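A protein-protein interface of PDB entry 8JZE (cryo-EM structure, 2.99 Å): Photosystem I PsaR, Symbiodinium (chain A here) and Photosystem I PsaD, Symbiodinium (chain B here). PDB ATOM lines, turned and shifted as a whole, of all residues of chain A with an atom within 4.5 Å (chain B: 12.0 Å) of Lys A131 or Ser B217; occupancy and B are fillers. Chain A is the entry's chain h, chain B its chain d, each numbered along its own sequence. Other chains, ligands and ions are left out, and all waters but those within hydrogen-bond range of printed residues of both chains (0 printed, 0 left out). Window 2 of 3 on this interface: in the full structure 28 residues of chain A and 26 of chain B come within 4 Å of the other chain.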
ATOM      1  N   SER A  54       4.430  -4.483  -5.538  1.00  0.00           N
ATOM      2  CA  SER A  54       5.818  -4.927  -5.549  1.00  0.00           C
ATOM      3  C   SER A  54       6.538  -4.548  -6.836  1.00  0.00           C
ATOM      4  O   SER A  54       7.768  -4.453  -6.840  1.00  0.00           O
ATOM      5  CB  SER A  54       5.887  -6.437  -5.343  1.00  0.00           C
ATOM      6  OG  SER A  54       5.119  -6.827  -4.220  1.00  0.00           O
ATOM      7  N   HIS A  55       5.799  -4.323  -7.923  1.00  0.00           N
ATOM      8  CA  HIS A  55       6.407  -3.982  -9.203  1.00  0.00           C
ATOM      9  C   HIS A  55       6.992  -2.576  -9.231  1.00  0.00           C
ATOM     10  O   HIS A  55       7.676  -2.231 -10.200  1.00  0.00           O
ATOM     11  CB  HIS A  55       5.378  -4.138 -10.323  1.00  0.00           C
ATOM     12  CG  HIS A  55       4.973  -5.557 -10.585  1.00  0.00           C
ATOM     13  ND1 HIS A  55       4.003  -6.203  -9.851  1.00  0.00           N
ATOM     14  CD2 HIS A  55       5.408  -6.452 -11.503  1.00  0.00           C
ATOM     15  CE1 HIS A  55       3.857  -7.435 -10.305  1.00  0.00           C
ATOM     16  NE2 HIS A  55       4.698  -7.611 -11.308  1.00  0.00           N
ATOM     17  N   LYS A  61      11.735  -6.416  -6.985  1.00  0.00           N
ATOM     18  CA  LYS A  61      10.434  -6.955  -6.597  1.00  0.00           C
ATOM     19  C   LYS A  61      10.547  -8.363  -6.031  1.00  0.00           C
ATOM     20  O   LYS A  61       9.707  -8.777  -5.225  1.00  0.00           O
ATOM     21  CB  LYS A  61       9.480  -6.942  -7.794  1.00  0.00           C
ATOM     22  CG  LYS A  61       9.948  -7.768  -8.982  1.00  0.00           C
ATOM     23  CD  LYS A  61       8.941  -7.717 -10.120  1.00  0.00           C
ATOM     24  CE  LYS A  61       9.483  -8.388 -11.375  1.00  0.00           C
ATOM     25  NZ  LYS A  61      10.683  -7.686 -11.905  1.00  0.00           N
ATOM     26  N   SER A  64      13.404 -10.189  -0.704  1.00  0.00           N
ATOM     27  CA  SER A  64      12.658 -10.304   0.537  1.00  0.00           C
ATOM     28  C   SER A  64      12.768  -9.014   1.342  1.00  0.00           C
ATOM     29  O   SER A  64      13.679  -8.206   1.151  1.00  0.00           O
ATOM     30  CB  SER A  64      13.164 -11.484   1.367  1.00  0.00           C
ATOM     31  OG  SER A  64      12.491 -11.555   2.613  1.00  0.00           O
ATOM     32  N   SER A  65      11.811  -8.825   2.253  1.00  0.00           N
ATOM     33  CA  SER A  65      11.838  -7.647   3.113  1.00  0.00           C
ATOM     34  C   SER A  65      13.058  -7.661   4.026  1.00  0.00           C
ATOM     35  O   SER A  65      13.665  -6.615   4.276  1.00  0.00           O
ATOM     36  CB  SER A  65      10.550  -7.564   3.930  1.00  0.00           C
ATOM     37  OG  SER A  65      10.279  -8.795   4.574  1.00  0.00           O
ATOM     38  N   GLN A 126       8.182  -3.542   0.286  1.00  0.00           N
ATOM     39  CA  GLN A 126       8.089  -4.999   0.294  1.00  0.00           C
ATOM     40  C   GLN A 126       7.368  -5.505   1.536  1.00  0.00           C
ATOM     41  O   GLN A 126       6.564  -6.441   1.457  1.00  0.00           O
ATOM     42  CB  GLN A 126       9.483  -5.621   0.204  1.00  0.00           C
ATOM     43  CG  GLN A 126      10.040  -5.718  -1.203  1.00  0.00           C
ATOM     44  CD  GLN A 126       9.257  -6.672  -2.083  1.00  0.00           C
ATOM     45  OE1 GLN A 126       8.230  -6.307  -2.655  1.00  0.00           O
ATOM     46  NE2 GLN A 126       9.738  -7.903  -2.198  1.00  0.00           N
ATOM     47  N   ASN A 129       3.518  -5.278   1.313  1.00  0.00           N
ATOM     48  CA  ASN A 129       2.903  -6.275   0.449  1.00  0.00           C
ATOM     49  C   ASN A 129       3.061  -7.697   0.971  1.00  0.00           C
ATOM     50  O   ASN A 129       2.564  -8.631   0.334  1.00  0.00           O
ATOM     51  CB  ASN A 129       3.489  -6.177  -0.963  1.00  0.00           C
ATOM     52  CG  ASN A 129       3.276  -4.812  -1.589  1.00  0.00           C
ATOM     53  OD1 ASN A 129       2.283  -4.579  -2.275  1.00  0.00           O
ATOM     54  ND2 ASN A 129       4.212  -3.901  -1.353  1.00  0.00           N
ATOM     55  N   GLY A 130       3.738  -7.886   2.101  1.00  0.00           N
ATOM     56  CA  GLY A 130       3.895  -9.199   2.687  1.00  0.00           C
ATOM     57  C   GLY A 130       4.994 -10.045   2.089  1.00  0.00           C
ATOM     58  O   GLY A 130       5.176 -11.190   2.524  1.00  0.00           O
ATOM     59  N   LYS A 131       5.733  -9.528   1.113  1.00  0.00           N
ATOM     60  CA  LYS A 131       6.823 -10.270   0.495  1.00  0.00           C
ATOM     61  C   LYS A 131       8.001 -10.413   1.451  1.00  0.00           C
ATOM     62  O   LYS A 131       8.038  -9.784   2.509  1.00  0.00           O
ATOM     63  CB  LYS A 131       7.273  -9.585  -0.797  1.00  0.00           C
ATOM     64  CG  LYS A 131       6.723 -10.215  -2.067  1.00  0.00           C
ATOM     65  CD  LYS A 131       5.205 -10.265  -2.060  1.00  0.00           C
ATOM     66  CE  LYS A 131       4.674 -11.056  -3.245  1.00  0.00           C
ATOM     67  NZ  LYS A 131       3.188 -11.143  -3.234  1.00  0.00           N
ATOM     68  OXT LYS A 131       8.941 -11.162   1.188  1.00  0.00           O
ATOM     69  N   ASP B 209      -2.999 -13.105 -20.470  1.00  0.00           N
ATOM     70  CA  ASP B 209      -1.550 -12.994 -20.337  1.00  0.00           C
ATOM     71  C   ASP B 209      -1.172 -11.927 -19.318  1.00  0.00           C
ATOM     72  O   ASP B 209      -0.261 -12.130 -18.507  1.00  0.00           O
ATOM     73  CB  ASP B 209      -0.926 -12.682 -21.697  1.00  0.00           C
ATOM     74  CG  ASP B 209       0.591 -12.674 -21.660  1.00  0.00           C
ATOM     75  OD1 ASP B 209       1.175 -13.237 -20.709  1.00  0.00           O
ATOM     76  OD2 ASP B 209       1.201 -12.100 -22.584  1.00  0.00           O
ATOM     77  N   ARG B 210      -1.859 -10.784 -19.348  1.00  0.00           N
ATOM     78  CA  ARG B 210      -1.558  -9.719 -18.395  1.00  0.00           C
ATOM     79  C   ARG B 210      -1.869 -10.149 -16.968  1.00  0.00           C
ATOM     80  O   ARG B 210      -1.102  -9.855 -16.045  1.00  0.00           O
ATOM     81  CB  ARG B 210      -2.331  -8.454 -18.759  1.00  0.00           C
ATOM     82  CG  ARG B 210      -1.871  -7.822 -20.053  1.00  0.00           C
ATOM     83  CD  ARG B 210      -2.681  -6.591 -20.400  1.00  0.00           C
ATOM     84  NE  ARG B 210      -2.202  -5.975 -21.631  1.00  0.00           N
ATOM     85  CZ  ARG B 210      -2.685  -4.853 -22.143  1.00  0.00           C
ATOM     86  NH1 ARG B 210      -3.672  -4.196 -21.558  1.00  0.00           N
ATOM     87  NH2 ARG B 210      -2.164  -4.377 -23.270  1.00  0.00           N
ATOM     88  N   ALA B 211      -2.992 -10.844 -16.764  1.00  0.00           N
ATOM     89  CA  ALA B 211      -3.319 -11.334 -15.428  1.00  0.00           C
ATOM     90  C   ALA B 211      -2.281 -12.340 -14.944  1.00  0.00           C
ATOM     91  O   ALA B 211      -1.851 -12.291 -13.784  1.00  0.00           O
ATOM     92  CB  ALA B 211      -4.714 -11.956 -15.423  1.00  0.00           C
ATOM     93  N   ALA B 212      -1.861 -13.254 -15.823  1.00  0.00           N
ATOM     94  CA  ALA B 212      -0.856 -14.241 -15.441  1.00  0.00           C
ATOM     95  C   ALA B 212       0.466 -13.574 -15.086  1.00  0.00           C
ATOM     96  O   ALA B 212       1.120 -13.957 -14.109  1.00  0.00           O
ATOM     97  CB  ALA B 212      -0.661 -15.254 -16.570  1.00  0.00           C
ATOM     98  N   LYS B 213       0.880 -12.578 -15.872  1.00  0.00           N
ATOM     99  CA  LYS B 213       2.126 -11.875 -15.584  1.00  0.00           C
ATOM    100  C   LYS B 213       2.031 -11.082 -14.287  1.00  0.00           C
ATOM    101  O   LYS B 213       2.987 -11.050 -13.503  1.00  0.00           O
ATOM    102  CB  LYS B 213       2.491 -10.957 -16.750  1.00  0.00           C
ATOM    103  CG  LYS B 213       2.905 -11.693 -18.013  1.00  0.00           C
ATOM    104  CD  LYS B 213       3.166 -10.725 -19.156  1.00  0.00           C
ATOM    105  CE  LYS B 213       4.131  -9.626 -18.738  1.00  0.00           C
ATOM    106  NZ  LYS B 213       5.403 -10.178 -18.195  1.00  0.00           N
ATOM    107  N   ALA B 214       0.890 -10.433 -14.044  1.00  0.00           N
ATOM    108  CA  ALA B 214       0.723  -9.663 -12.818  1.00  0.00           C
ATOM    109  C   ALA B 214       0.727 -10.568 -11.595  1.00  0.00           C
ATOM    110  O   ALA B 214       1.240 -10.186 -10.536  1.00  0.00           O
ATOM    111  CB  ALA B 214      -0.567  -8.848 -12.880  1.00  0.00           C
ATOM    112  N   ALA B 215       0.165 -11.771 -11.716  1.00  0.00           N
ATOM    113  CA  ALA B 215       0.139 -12.693 -10.588  1.00  0.00           C
ATOM    114  C   ALA B 215       1.451 -13.461 -10.471  1.00  0.00           C
ATOM    115  O   ALA B 215       1.449 -14.693 -10.392  1.00  0.00           O
ATOM    116  CB  ALA B 215      -1.036 -13.665 -10.720  1.00  0.00           C
ATOM    117  N   LYS B 216       2.569 -12.740 -10.452  1.00  0.00           N
ATOM    118  CA  LYS B 216       3.894 -13.317 -10.250  1.00  0.00           C
ATOM    119  C   LYS B 216       4.644 -12.682  -9.092  1.00  0.00           C
ATOM    120  O   LYS B 216       5.334 -13.386  -8.349  1.00  0.00           O
ATOM    121  CB  LYS B 216       4.738 -13.186 -11.528  1.00  0.00           C
ATOM    122  CG  LYS B 216       4.222 -13.986 -12.712  1.00  0.00           C
ATOM    123  CD  LYS B 216       5.174 -13.894 -13.896  1.00  0.00           C
ATOM    124  CE  LYS B 216       6.547 -14.452 -13.552  1.00  0.00           C
ATOM    125  NZ  LYS B 216       6.490 -15.894 -13.184  1.00  0.00           N
ATOM    126  N   SER B 217       4.527 -11.365  -8.922  1.00  0.00           N
ATOM    127  CA  SER B 217       5.141 -10.666  -7.804  1.00  0.00           C
ATOM    128  C   SER B 217       4.173  -9.775  -7.040  1.00  0.00           C
ATOM    129  O   SER B 217       4.538  -9.286  -5.966  1.00  0.00           O
ATOM    130  CB  SER B 217       6.323  -9.811  -8.285  1.00  0.00           C
ATOM    131  OG  SER B 217       7.255 -10.596  -9.006  1.00  0.00           O
ATOM    132  N   LEU B 218       2.969  -9.544  -7.554  1.00  0.00           N
ATOM    133  CA  LEU B 218       1.974  -8.721  -6.877  1.00  0.00           C
ATOM    134  C   LEU B 218       1.523  -9.362  -5.569  1.00  0.00           C
ATOM    135  O   LEU B 218       1.398  -8.688  -4.546  1.00  0.00           O
ATOM    136  CB  LEU B 218       0.768  -8.484  -7.788  1.00  0.00           C
ATOM    137  CG  LEU B 218      -0.448  -7.792  -7.168  1.00  0.00           C
ATOM    138  CD1 LEU B 218      -0.071  -6.425  -6.634  1.00  0.00           C
ATOM    139  CD2 LEU B 218      -1.580  -7.681  -8.176  1.00  0.00           C
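Lys A131 touches just these residues of chain B: Ser B217 and Leu B218. Ser B217 touches just these residues of chain A: Ser A54, His A55, Lys A61 and Lys A131. Ser A54 touches one residue of chain B. His A55 touches three residues of chain B. No residue of chain B comes within 4 Å of Ser A64. No residue of chain B comes within 4 Å of Gln A126. No residue of chain B comes within 4 Å of Asn A129. No residue of chain B comes within 4 Å of Gly A130. Printed residues of chain A within 4 Å of Ala B214: His A55. Of the printed residues of chain A, Leu B218 touches His A55 and Lys A131. Asp B209 touches none of the printed residues of chain A. Lys B216 touches none of the printed residues of chain A. The nearest printed residue of chain A that does not touch Ser B217 is Gln A126 (5.8 Å). The nearest printed residue of chain A that does not touch Ala B214 is Lys A131 (7.6 Å).
The backbone carbonyl oxygen (O) of Gln A126 is in hydrogen-bond range of the backbone NH (N) of Lys A131, at 3.2 Å. O of Lys A131 lies within hydrogen-bond range of OG of Ser A65 (3.2 Å). The backbone carbonyl oxygen (O) of Lys A61 is in hydrogen-bond range of the side-chain amide nitrogen (NE2) of Gln A126, at 3.2 Å.
O of Ala B214 touches CE1 of His A55, 3.8 Å away. Ser B217 touches His A55 (CB to CE1, 3.98 Å). Leu B218 touches His A55. Ser B217 touches Lys A61. Ser B217 touches Lys A131.
NZ of Lys A131 lies within hydrogen-bond range of O of Leu B218 (3.3 Å). O of Ser B217 sits at hydrogen-bond distance from OG of Ser A54 (3.1 Å).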
